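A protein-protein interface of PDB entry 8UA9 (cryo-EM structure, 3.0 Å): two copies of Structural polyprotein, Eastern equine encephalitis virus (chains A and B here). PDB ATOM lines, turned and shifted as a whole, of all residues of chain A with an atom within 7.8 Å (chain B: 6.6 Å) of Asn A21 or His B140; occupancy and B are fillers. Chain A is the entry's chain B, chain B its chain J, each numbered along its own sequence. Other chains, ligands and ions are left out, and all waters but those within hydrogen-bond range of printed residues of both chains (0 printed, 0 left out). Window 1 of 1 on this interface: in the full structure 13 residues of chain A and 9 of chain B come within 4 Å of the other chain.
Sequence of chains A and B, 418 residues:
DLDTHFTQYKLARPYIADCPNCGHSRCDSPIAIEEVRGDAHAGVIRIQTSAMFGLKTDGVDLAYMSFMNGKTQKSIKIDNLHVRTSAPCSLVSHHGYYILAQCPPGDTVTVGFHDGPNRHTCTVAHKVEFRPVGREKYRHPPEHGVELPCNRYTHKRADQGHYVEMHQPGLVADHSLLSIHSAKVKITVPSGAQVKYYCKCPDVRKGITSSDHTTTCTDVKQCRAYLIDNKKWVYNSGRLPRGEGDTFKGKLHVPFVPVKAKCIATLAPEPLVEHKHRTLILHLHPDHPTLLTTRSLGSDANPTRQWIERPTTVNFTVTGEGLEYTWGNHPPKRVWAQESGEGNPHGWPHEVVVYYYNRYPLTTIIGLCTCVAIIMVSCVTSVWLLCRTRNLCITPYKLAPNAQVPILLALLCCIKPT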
ATOM      1  N   ASP A  18      -7.383   7.725  36.876  1.00  0.00           N
ATOM      2  CA  ASP A  18      -7.004   6.689  35.936  1.00  0.00           C
ATOM      3  C   ASP A  18      -8.181   6.353  35.057  1.00  0.00           C
ATOM      4  O   ASP A  18      -9.316   6.305  35.526  1.00  0.00           O
ATOM      5  CB  ASP A  18      -6.604   5.426  36.681  1.00  0.00           C
ATOM      6  CG  ASP A  18      -6.797   4.176  35.854  1.00  0.00           C
ATOM      7  OD1 ASP A  18      -6.421   4.154  34.662  1.00  0.00           O
ATOM      8  OD2 ASP A  18      -7.434   3.240  36.371  1.00  0.00           O
ATOM      9  N   CYS A  19      -7.916   6.147  33.769  1.00  0.00           N
ATOM     10  CA  CYS A  19      -8.982   5.740  32.885  1.00  0.00           C
ATOM     11  C   CYS A  19      -8.475   4.774  31.826  1.00  0.00           C
ATOM     12  O   CYS A  19      -7.364   4.965  31.302  1.00  0.00           O
ATOM     13  CB  CYS A  19      -9.603   6.967  32.246  1.00  0.00           C
ATOM     14  SG  CYS A  19      -9.687   7.027  30.494  1.00  0.00           S
ATOM     15  N   PRO A  20      -9.252   3.715  31.509  1.00  0.00           N
ATOM     16  CA  PRO A  20      -8.673   2.561  30.819  1.00  0.00           C
ATOM     17  C   PRO A  20      -8.210   2.792  29.401  1.00  0.00           C
ATOM     18  O   PRO A  20      -7.179   2.257  28.999  1.00  0.00           O
ATOM     19  CB  PRO A  20      -9.800   1.529  30.854  1.00  0.00           C
ATOM     20  CG  PRO A  20     -10.965   2.191  31.345  1.00  0.00           C
ATOM     21  CD  PRO A  20     -10.712   3.593  31.605  1.00  0.00           C
ATOM     22  N   ASN A  21      -9.023   3.466  28.607  1.00  0.00           N
ATOM     23  CA  ASN A  21      -8.747   3.738  27.202  1.00  0.00           C
ATOM     24  C   ASN A  21      -8.648   5.240  26.997  1.00  0.00           C
ATOM     25  O   ASN A  21      -9.660   5.941  26.983  1.00  0.00           O
ATOM     26  CB  ASN A  21      -9.801   3.114  26.301  1.00  0.00           C
ATOM     27  CG  ASN A  21      -9.221   2.438  25.070  1.00  0.00           C
ATOM     28  OD1 ASN A  21      -8.013   2.292  24.911  1.00  0.00           O
ATOM     29  ND2 ASN A  21     -10.106   2.022  24.177  1.00  0.00           N
ATOM     30  N   CYS A  22      -7.433   5.731  26.858  1.00  0.00           N
ATOM     31  CA  CYS A  22      -7.165   7.126  26.585  1.00  0.00           C
ATOM     32  C   CYS A  22      -7.003   7.386  25.106  1.00  0.00           C
ATOM     33  O   CYS A  22      -6.616   8.490  24.725  1.00  0.00           O
ATOM     34  CB  CYS A  22      -5.891   7.561  27.279  1.00  0.00           C
ATOM     35  SG  CYS A  22      -6.074   8.809  28.448  1.00  0.00           S
ATOM     36  N   GLY A  23      -7.267   6.394  24.266  1.00  0.00           N
ATOM     37  CA  GLY A  23      -6.687   6.357  22.948  1.00  0.00           C
ATOM     38  C   GLY A  23      -5.589   5.323  22.898  1.00  0.00           C
ATOM     39  O   GLY A  23      -5.864   4.121  22.837  1.00  0.00           O
ATOM     40  N   HIS A  24      -4.349   5.805  22.869  1.00  0.00           N
ATOM     41  CA  HIS A  24      -3.170   4.950  22.804  1.00  0.00           C
ATOM     42  C   HIS A  24      -3.248   3.802  23.809  1.00  0.00           C
ATOM     43  O   HIS A  24      -3.237   2.629  23.425  1.00  0.00           O
ATOM     44  CB  HIS A  24      -1.932   5.817  23.054  1.00  0.00           C
ATOM     45  CG  HIS A  24      -0.695   5.338  22.376  1.00  0.00           C
ATOM     46  ND1 HIS A  24      -0.050   4.176  22.736  1.00  0.00           N
ATOM     47  CD2 HIS A  24       0.046   5.891  21.389  1.00  0.00           C
ATOM     48  CE1 HIS A  24       1.022   4.019  21.980  1.00  0.00           C
ATOM     49  NE2 HIS A  24       1.102   5.045  21.153  1.00  0.00           N
ATOM     50  N   SER A  25      -3.368   4.115  25.095  1.00  0.00           N
ATOM     51  CA  SER A  25      -3.303   3.108  26.147  1.00  0.00           C
ATOM     52  C   SER A  25      -4.021   3.655  27.375  1.00  0.00           C
ATOM     53  O   SER A  25      -4.733   4.654  27.293  1.00  0.00           O
ATOM     54  CB  SER A  25      -1.843   2.734  26.411  1.00  0.00           C
ATOM     55  OG  SER A  25      -1.039   3.899  26.452  1.00  0.00           O
ATOM     56  N   ARG A  26      -3.869   2.979  28.508  1.00  0.00           N
ATOM     57  CA  ARG A  26      -4.508   3.372  29.757  1.00  0.00           C
ATOM     58  C   ARG A  26      -3.738   4.514  30.395  1.00  0.00           C
ATOM     59  O   ARG A  26      -2.510   4.484  30.437  1.00  0.00           O
ATOM     60  CB  ARG A  26      -4.559   2.142  30.664  1.00  0.00           C
ATOM     61  CG  ARG A  26      -4.941   2.311  32.103  1.00  0.00           C
ATOM     62  CD  ARG A  26      -4.695   1.035  32.873  1.00  0.00           C
ATOM     63  NE  ARG A  26      -5.761   0.053  32.774  1.00  0.00           N
ATOM     64  CZ  ARG A  26      -6.860   0.044  33.513  1.00  0.00           C
ATOM     65  NH1 ARG A  26      -7.144   1.028  34.346  1.00  0.00           N
ATOM     66  NH2 ARG A  26      -7.706  -0.970  33.399  1.00  0.00           N
ATOM     67  N   CYS A  27      -4.455   5.539  30.872  1.00  0.00           N
ATOM     68  CA  CYS A  27      -3.792   6.788  31.218  1.00  0.00           C
ATOM     69  C   CYS A  27      -4.242   7.207  32.602  1.00  0.00           C
ATOM     70  O   CYS A  27      -5.052   6.541  33.247  1.00  0.00           O
ATOM     71  CB  CYS A  27      -4.206   7.928  30.276  1.00  0.00           C
ATOM     72  SG  CYS A  27      -5.935   7.808  29.793  1.00  0.00           S
ATOM     73  N   SER A  29      -6.240  10.490  33.175  1.00  0.00           N
ATOM     74  CA  SER A  29      -6.866  11.499  32.345  1.00  0.00           C
ATOM     75  C   SER A  29      -7.527  12.589  33.182  1.00  0.00           C
ATOM     76  O   SER A  29      -7.899  12.352  34.334  1.00  0.00           O
ATOM     77  CB  SER A  29      -7.929  10.873  31.452  1.00  0.00           C
ATOM     78  OG  SER A  29      -8.888  10.184  32.225  1.00  0.00           O
ATOM     79  N   ILE A  31     -10.374  13.755  32.184  1.00  0.00           N
ATOM     80  CA  ILE A  31     -11.766  13.581  31.805  1.00  0.00           C
ATOM     81  C   ILE A  31     -12.211  12.174  32.174  1.00  0.00           C
ATOM     82  O   ILE A  31     -13.080  11.595  31.513  1.00  0.00           O
ATOM     83  CB  ILE A  31     -11.979  13.901  30.318  1.00  0.00           C
ATOM     84  CG1 ILE A  31     -13.470  14.074  30.021  1.00  0.00           C
ATOM     85  CG2 ILE A  31     -11.341  12.842  29.425  1.00  0.00           C
ATOM     86  CD1 ILE A  31     -13.925  15.466  30.033  1.00  0.00           C
ATOM     87  N   ILE A  33     -13.998   9.061  33.290  1.00  0.00           N
ATOM     88  CA  ILE A  33     -15.418   8.818  33.503  1.00  0.00           C
ATOM     89  C   ILE A  33     -15.564   8.013  34.781  1.00  0.00           C
ATOM     90  O   ILE A  33     -15.062   6.893  34.879  1.00  0.00           O
ATOM     91  CB  ILE A  33     -16.039   8.076  32.315  1.00  0.00           C
ATOM     92  CG1 ILE A  33     -16.067   8.958  31.078  1.00  0.00           C
ATOM     93  CG2 ILE A  33     -17.436   7.625  32.642  1.00  0.00           C
ATOM     94  CD1 ILE A  33     -16.033   8.192  29.808  1.00  0.00           C
ATOM     95  N   THR A  85     -21.205   7.268  22.022  1.00  0.00           N
ATOM     96  CA  THR A  85     -21.287   5.856  22.392  1.00  0.00           C
ATOM     97  C   THR A  85     -20.892   4.903  21.274  1.00  0.00           C
ATOM     98  O   THR A  85     -19.974   4.095  21.424  1.00  0.00           O
ATOM     99  CB  THR A  85     -22.716   5.522  22.818  1.00  0.00           C
ATOM    100  OG1 THR A  85     -23.631   6.000  21.835  1.00  0.00           O
ATOM    101  CG2 THR A  85     -23.031   6.140  24.135  1.00  0.00           C
ATOM    102  N   ASP A 107     -21.938   0.138  23.105  1.00  0.00           N
ATOM    103  CA  ASP A 107     -21.220  -0.703  24.051  1.00  0.00           C
ATOM    104  C   ASP A 107     -20.065   0.011  24.726  1.00  0.00           C
ATOM    105  O   ASP A 107     -19.370  -0.604  25.531  1.00  0.00           O
ATOM    106  CB  ASP A 107     -20.684  -1.938  23.332  1.00  0.00           C
ATOM    107  CG  ASP A 107     -21.782  -2.826  22.802  1.00  0.00           C
ATOM    108  OD1 ASP A 107     -22.967  -2.538  23.065  1.00  0.00           O
ATOM    109  OD2 ASP A 107     -21.465  -3.804  22.095  1.00  0.00           O
ATOM    110  N   THR A 108     -19.816   1.269  24.391  1.00  0.00           N
ATOM    111  CA  THR A 108     -18.791   2.090  25.005  1.00  0.00           C
ATOM    112  C   THR A 108     -19.373   3.468  25.242  1.00  0.00           C
ATOM    113  O   THR A 108     -20.410   3.813  24.679  1.00  0.00           O
ATOM    114  CB  THR A 108     -17.548   2.198  24.135  1.00  0.00           C
ATOM    115  OG1 THR A 108     -17.824   3.055  23.024  1.00  0.00           O
ATOM    116  CG2 THR A 108     -17.142   0.855  23.613  1.00  0.00           C
ATOM    117  N   VAL A 109     -18.744   4.237  26.122  1.00  0.00           N
ATOM    118  CA  VAL A 109     -19.062   5.647  26.288  1.00  0.00           C
ATOM    119  C   VAL A 109     -17.760   6.418  26.309  1.00  0.00           C
ATOM    120  O   VAL A 109     -16.920   6.178  27.177  1.00  0.00           O
ATOM    121  CB  VAL A 109     -19.868   5.910  27.562  1.00  0.00           C
ATOM    122  CG1 VAL A 109     -20.555   7.223  27.469  1.00  0.00           C
ATOM    123  CG2 VAL A 109     -20.878   4.829  27.775  1.00  0.00           C
ATOM    124  N   THR A 110     -17.580   7.325  25.354  1.00  0.00           N
ATOM    125  CA  THR A 110     -16.365   8.110  25.225  1.00  0.00           C
ATOM    126  C   THR A 110     -16.671   9.578  25.419  1.00  0.00           C
ATOM    127  O   THR A 110     -17.622  10.089  24.831  1.00  0.00           O
ATOM    128  CB  THR A 110     -15.725   7.925  23.858  1.00  0.00           C
ATOM    129  OG1 THR A 110     -15.616   6.531  23.561  1.00  0.00           O
ATOM    130  CG2 THR A 110     -14.357   8.583  23.803  1.00  0.00           C
ATOM    131  N   VAL A 111     -15.867  10.247  26.235  1.00  0.00           N
ATOM    132  CA  VAL A 111     -15.975  11.679  26.461  1.00  0.00           C
ATOM    133  C   VAL A 111     -14.627  12.291  26.164  1.00  0.00           C
ATOM    134  O   VAL A 111     -13.602  11.749  26.577  1.00  0.00           O
ATOM    135  CB  VAL A 111     -16.415  11.996  27.895  1.00  0.00           C
ATOM    136  CG1 VAL A 111     -16.678  13.480  28.047  1.00  0.00           C
ATOM    137  CG2 VAL A 111     -17.646  11.213  28.241  1.00  0.00           C
ATOM    138  N   THR A 121      -9.181  12.344  25.780  1.00  0.00           N
ATOM    139  CA  THR A 121     -10.304  11.469  25.484  1.00  0.00           C
ATOM    140  C   THR A 121     -10.302  10.283  26.433  1.00  0.00           C
ATOM    141  O   THR A 121      -9.234   9.804  26.811  1.00  0.00           O
ATOM    142  CB  THR A 121     -10.267  10.992  24.038  1.00  0.00           C
ATOM    143  OG1 THR A 121     -11.162   9.890  23.881  1.00  0.00           O
ATOM    144  CG2 THR A 121      -8.871  10.561  23.638  1.00  0.00           C
ATOM    145  N   CYS A 122     -11.482   9.827  26.843  1.00  0.00           N
ATOM    146  CA  CYS A 122     -11.583   8.666  27.717  1.00  0.00           C
ATOM    147  C   CYS A 122     -12.808   7.844  27.376  1.00  0.00           C
ATOM    148  O   CYS A 122     -13.923   8.364  27.387  1.00  0.00           O
ATOM    149  CB  CYS A 122     -11.654   9.084  29.172  1.00  0.00           C
ATOM    150  SG  CYS A 122     -11.779   7.695  30.253  1.00  0.00           S
ATOM    151  N   THR A 123     -12.581   6.559  27.104  1.00  0.00           N
ATOM    152  CA  THR A 123     -13.586   5.591  26.688  1.00  0.00           C
ATOM    153  C   THR A 123     -13.738   4.510  27.751  1.00  0.00           C
ATOM    154  O   THR A 123     -12.775   3.811  28.062  1.00  0.00           O
ATOM    155  CB  THR A 123     -13.216   4.963  25.351  1.00  0.00           C
ATOM    156  OG1 THR A 123     -13.211   5.966  24.336  1.00  0.00           O
ATOM    157  CG2 THR A 123     -14.239   3.923  24.948  1.00  0.00           C
ATOM    158  N   VAL A 124     -14.936   4.385  28.303  1.00  0.00           N
ATOM    159  CA  VAL A 124     -15.293   3.335  29.251  1.00  0.00           C
ATOM    160  C   VAL A 124     -16.186   2.354  28.525  1.00  0.00           C
ATOM    161  O   VAL A 124     -16.612   2.616  27.399  1.00  0.00           O
ATOM    162  CB  VAL A 124     -15.979   3.863  30.518  1.00  0.00           C
ATOM    163  CG1 VAL A 124     -15.001   4.656  31.329  1.00  0.00           C
ATOM    164  CG2 VAL A 124     -17.205   4.692  30.204  1.00  0.00           C
ATOM    165  N   ALA A 125     -16.457   1.215  29.148  1.00  0.00           N
ATOM    166  CA  ALA A 125     -17.093   0.084  28.498  1.00  0.00           C
ATOM    167  C   ALA A 125     -18.469  -0.178  29.084  1.00  0.00           C
ATOM    168  O   ALA A 125     -18.948  -1.305  29.095  1.00  0.00           O
ATOM    169  CB  ALA A 125     -16.229  -1.159  28.628  1.00  0.00           C
ATOM    170  N   HIS A 126     -19.109   0.869  29.571  1.00  0.00           N
ATOM    171  CA  HIS A 126     -20.516   0.825  29.922  1.00  0.00           C
ATOM    172  C   HIS A 126     -21.376   0.651  28.689  1.00  0.00           C
ATOM    173  O   HIS A 126     -21.232   1.392  27.716  1.00  0.00           O
ATOM    174  CB  HIS A 126     -20.917   2.091  30.654  1.00  0.00           C
ATOM    175  CG  HIS A 126     -22.244   1.990  31.313  1.00  0.00           C
ATOM    176  ND1 HIS A 126     -22.445   1.253  32.455  1.00  0.00           N
ATOM    177  CD2 HIS A 126     -23.446   2.499  30.976  1.00  0.00           C
ATOM    178  CE1 HIS A 126     -23.714   1.331  32.805  1.00  0.00           C
ATOM    179  NE2 HIS A 126     -24.343   2.081  31.923  1.00  0.00           N
ATOM    180  N   SER B  90      -9.023   5.067  17.317  1.00  0.00           N
ATOM    181  CA  SER B  90      -7.987   5.742  18.074  1.00  0.00           C
ATOM    182  C   SER B  90      -6.642   5.462  17.435  1.00  0.00           C
ATOM    183  O   SER B  90      -6.197   4.313  17.422  1.00  0.00           O
ATOM    184  CB  SER B  90      -7.997   5.268  19.519  1.00  0.00           C
ATOM    185  OG  SER B  90      -9.322   5.137  19.989  1.00  0.00           O
ATOM    186  N   GLN B 102      -7.010   1.374  17.181  1.00  0.00           N
ATOM    187  CA  GLN B 102      -7.996   0.603  17.929  1.00  0.00           C
ATOM    188  C   GLN B 102      -9.378   0.920  17.395  1.00  0.00           C
ATOM    189  O   GLN B 102      -9.804   2.075  17.461  1.00  0.00           O
ATOM    190  CB  GLN B 102      -7.934   0.933  19.412  1.00  0.00           C
ATOM    191  CG  GLN B 102      -6.836   0.234  20.174  1.00  0.00           C
ATOM    192  CD  GLN B 102      -7.327  -0.505  21.390  1.00  0.00           C
ATOM    193  OE1 GLN B 102      -8.444  -1.012  21.423  1.00  0.00           O
ATOM    194  NE2 GLN B 102      -6.487  -0.568  22.411  1.00  0.00           N
ATOM    195  N   PHE B 130     -14.234  -7.524  16.358  1.00  0.00           N
ATOM    196  CA  PHE B 130     -13.615  -7.468  17.662  1.00  0.00           C
ATOM    197  C   PHE B 130     -13.430  -8.889  18.154  1.00  0.00           C
ATOM    198  O   PHE B 130     -14.367  -9.690  18.121  1.00  0.00           O
ATOM    199  CB  PHE B 130     -14.474  -6.676  18.626  1.00  0.00           C
ATOM    200  CG  PHE B 130     -13.877  -6.505  19.968  1.00  0.00           C
ATOM    201  CD1 PHE B 130     -12.997  -5.496  20.217  1.00  0.00           C
ATOM    202  CD2 PHE B 130     -14.219  -7.330  20.991  1.00  0.00           C
ATOM    203  CE1 PHE B 130     -12.468  -5.335  21.454  1.00  0.00           C
ATOM    204  CE2 PHE B 130     -13.687  -7.159  22.225  1.00  0.00           C
ATOM    205  CZ  PHE B 130     -12.814  -6.162  22.450  1.00  0.00           C
ATOM    206  N   TYR B 138     -16.712 -10.301  25.718  1.00  0.00           N
ATOM    207  CA  TYR B 138     -16.872  -8.885  25.986  1.00  0.00           C
ATOM    208  C   TYR B 138     -16.670  -8.082  24.712  1.00  0.00           C
ATOM    209  O   TYR B 138     -15.938  -8.496  23.817  1.00  0.00           O
ATOM    210  CB  TYR B 138     -15.879  -8.445  27.051  1.00  0.00           C
ATOM    211  CG  TYR B 138     -14.433  -8.642  26.705  1.00  0.00           C
ATOM    212  CD1 TYR B 138     -13.726  -7.665  26.056  1.00  0.00           C
ATOM    213  CD2 TYR B 138     -13.761  -9.781  27.070  1.00  0.00           C
ATOM    214  CE1 TYR B 138     -12.416  -7.832  25.751  1.00  0.00           C
ATOM    215  CE2 TYR B 138     -12.456  -9.948  26.772  1.00  0.00           C
ATOM    216  CZ  TYR B 138     -11.785  -8.971  26.117  1.00  0.00           C
ATOM    217  OH  TYR B 138     -10.464  -9.134  25.810  1.00  0.00           O
ATOM    218  N   ARG B 139     -17.333  -6.928  24.628  1.00  0.00           N
ATOM    219  CA  ARG B 139     -17.304  -6.141  23.403  1.00  0.00           C
ATOM    220  C   ARG B 139     -16.294  -5.001  23.390  1.00  0.00           C
ATOM    221  O   ARG B 139     -15.901  -4.570  22.306  1.00  0.00           O
ATOM    222  CB  ARG B 139     -18.672  -5.521  23.115  1.00  0.00           C
ATOM    223  CG  ARG B 139     -19.877  -6.133  23.796  1.00  0.00           C
ATOM    224  CD  ARG B 139     -20.232  -7.459  23.216  1.00  0.00           C
ATOM    225  NE  ARG B 139     -20.955  -7.298  21.967  1.00  0.00           N
ATOM    226  CZ  ARG B 139     -22.223  -6.926  21.872  1.00  0.00           C
ATOM    227  NH1 ARG B 139     -22.952  -6.657  22.944  1.00  0.00           N
ATOM    228  NH2 ARG B 139     -22.778  -6.819  20.669  1.00  0.00           N
ATOM    229  N   HIS B 140     -15.880  -4.490  24.537  1.00  0.00           N
ATOM    230  CA  HIS B 140     -14.886  -3.447  24.701  1.00  0.00           C
ATOM    231  C   HIS B 140     -13.936  -3.892  25.799  1.00  0.00           C
ATOM    232  O   HIS B 140     -14.392  -4.558  26.731  1.00  0.00           O
ATOM    233  CB  HIS B 140     -15.502  -2.104  25.061  1.00  0.00           C
ATOM    234  CG  HIS B 140     -14.553  -0.962  24.923  1.00  0.00           C
ATOM    235  ND1 HIS B 140     -14.152  -0.479  23.700  1.00  0.00           N
ATOM    236  CD2 HIS B 140     -13.906  -0.220  25.847  1.00  0.00           C
ATOM    237  CE1 HIS B 140     -13.311   0.520  23.876  1.00  0.00           C
ATOM    238  NE2 HIS B 140     -13.140   0.694  25.171  1.00  0.00           N
ATOM    239  N   PRO B 141     -12.639  -3.608  25.733  1.00  0.00           N
ATOM    240  CA  PRO B 141     -11.737  -4.202  26.700  1.00  0.00           C
ATOM    241  C   PRO B 141     -12.022  -3.731  28.116  1.00  0.00           C
ATOM    242  O   PRO B 141     -12.193  -2.530  28.358  1.00  0.00           O
ATOM    243  CB  PRO B 141     -10.357  -3.728  26.250  1.00  0.00           C
ATOM    244  CG  PRO B 141     -10.504  -3.158  24.976  1.00  0.00           C
ATOM    245  CD  PRO B 141     -11.901  -3.023  24.607  1.00  0.00           C
ATOM    246  N   PRO B 142     -12.084  -4.647  29.078  1.00  0.00           N
ATOM    247  CA  PRO B 142     -12.466  -4.286  30.439  1.00  0.00           C
ATOM    248  C   PRO B 142     -11.385  -3.527  31.184  1.00  0.00           C
ATOM    249  O   PRO B 142     -10.207  -3.552  30.833  1.00  0.00           O
ATOM    250  CB  PRO B 142     -12.725  -5.636  31.088  1.00  0.00           C
ATOM    251  CG  PRO B 142     -11.802  -6.532  30.426  1.00  0.00           C
ATOM    252  CD  PRO B 142     -11.463  -5.977  29.079  1.00  0.00           C
ATOM    253  N   GLU B 143     -11.817  -2.830  32.228  1.00  0.00           N
ATOM    254  CA  GLU B 143     -10.900  -2.045  33.039  1.00  0.00           C
ATOM    255  C   GLU B 143     -10.183  -2.881  34.090  1.00  0.00           C
ATOM    256  O   GLU B 143      -9.059  -2.545  34.464  1.00  0.00           O
ATOM    257  CB  GLU B 143     -11.688  -0.930  33.726  1.00  0.00           C
ATOM    258  CG  GLU B 143     -11.082  -0.352  34.986  1.00  0.00           C
ATOM    259  CD  GLU B 143     -11.723   0.962  35.376  1.00  0.00           C
ATOM    260  OE1 GLU B 143     -12.946   1.109  35.173  1.00  0.00           O
ATOM    261  OE2 GLU B 143     -11.005   1.849  35.883  1.00  0.00           O
ATOM    262  N   THR B 266     -12.321 -10.043  30.831  1.00  0.00           N
ATOM    263  CA  THR B 266     -13.300  -9.922  31.890  1.00  0.00           C
ATOM    264  C   THR B 266     -13.266 -11.135  32.794  1.00  0.00           C
ATOM    265  O   THR B 266     -12.887 -12.233  32.388  1.00  0.00           O
ATOM    266  CB  THR B 266     -14.702  -9.788  31.322  1.00  0.00           C
ATOM    267  OG1 THR B 266     -14.878 -10.732  30.265  1.00  0.00           O
ATOM    268  CG2 THR B 266     -14.940  -8.415  30.800  1.00  0.00           C
ATOM    269  N   HIS B 288     -21.559 -10.792  30.271  1.00  0.00           N
ATOM    270  CA  HIS B 288     -21.407 -11.074  28.857  1.00  0.00           C
ATOM    271  C   HIS B 288     -21.477 -12.575  28.674  1.00  0.00           C
ATOM    272  O   HIS B 288     -21.302 -13.319  29.641  1.00  0.00           O
ATOM    273  CB  HIS B 288     -20.076 -10.557  28.312  1.00  0.00           C
ATOM    274  CG  HIS B 288     -19.651  -9.259  28.901  1.00  0.00           C
ATOM    275  ND1 HIS B 288     -20.096  -8.048  28.427  1.00  0.00           N
ATOM    276  CD2 HIS B 288     -18.799  -8.977  29.910  1.00  0.00           C
ATOM    277  CE1 HIS B 288     -19.545  -7.076  29.127  1.00  0.00           C
ATOM    278  NE2 HIS B 288     -18.756  -7.614  30.037  1.00  0.00           N
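ND2 of Asn A21 sits at hydrogen-bond distance from NE2 of His B140 (3.5 Å).
The side-chain carboxylate (OD2) of Asp A107 is in salt-bridge range of the guanidinium group (NH1) of Arg B139.
The guanidinium group of Arg A26 lies close to the backbone carbonyl oxygen of Glu B143.
O of Asn A21 lies within hydrogen-bond range of N of Thr A123, at 3.0 Å.
OG1 of Thr A108 is in hydrogen-bond range of O of Thr A85 (2.9 Å).
OG1 of Thr A110 lies within hydrogen-bond range of OG1 of Thr A123 (2.6 Å).
O of Ser B90 is in hydrogen-bond range of N of Gln B102 (3.1 Å).
The side-chain sulfur (SG) of Cys A19 is disulfide-bonded to the side-chain sulfur (SG) of Cys A122 (2.2 Å).
The side-chain sulfur of Cys A22 is disulfide-bonded to the side-chain sulfur of Cys A27.
Of chain A, only Asn A21, Thr A108, Thr A123 and Ala A125 come within 4 Å of His B140.
Of the printed residues of chain B, Asp A107 touches Arg B139 (3.2 Å).
Of the printed residues of chain A, Glu B143 touches Asp A18, Pro A20 and Arg A26.
Thr A110 touches none of the printed residues of chain B.
The nearest residue of chain B that does not touch Asn A21 is Gln B102 (4.1 Å).
Glu B143 touches Asp A18.
Glu B143 touches Pro A20 (CB to CG, 3.99 Å).
Gly A23 touches Ser B90 (CA to CB, 3.8 Å).
His B140 touches Thr A108.
CG2 of Thr A123 touches NE2 of His B140 (3.4 Å).
His B140 touches Ala A125.
Of the 25 printed residues of chain A, 9 touch a printed residue of chain B.
Of the 11 printed residues of chain B, 4 touch a printed residue of chain A.
Printed residues of chain B that touch a printed residue of chain A: Ser B90, Arg B139, His B140 and Glu B143.
Along chain B the printed residues that touch a printed residue of chain A span positions 90 to 143.
Among the printed residues, 9 pairs touch across the chains.
No position is printed for both chains.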
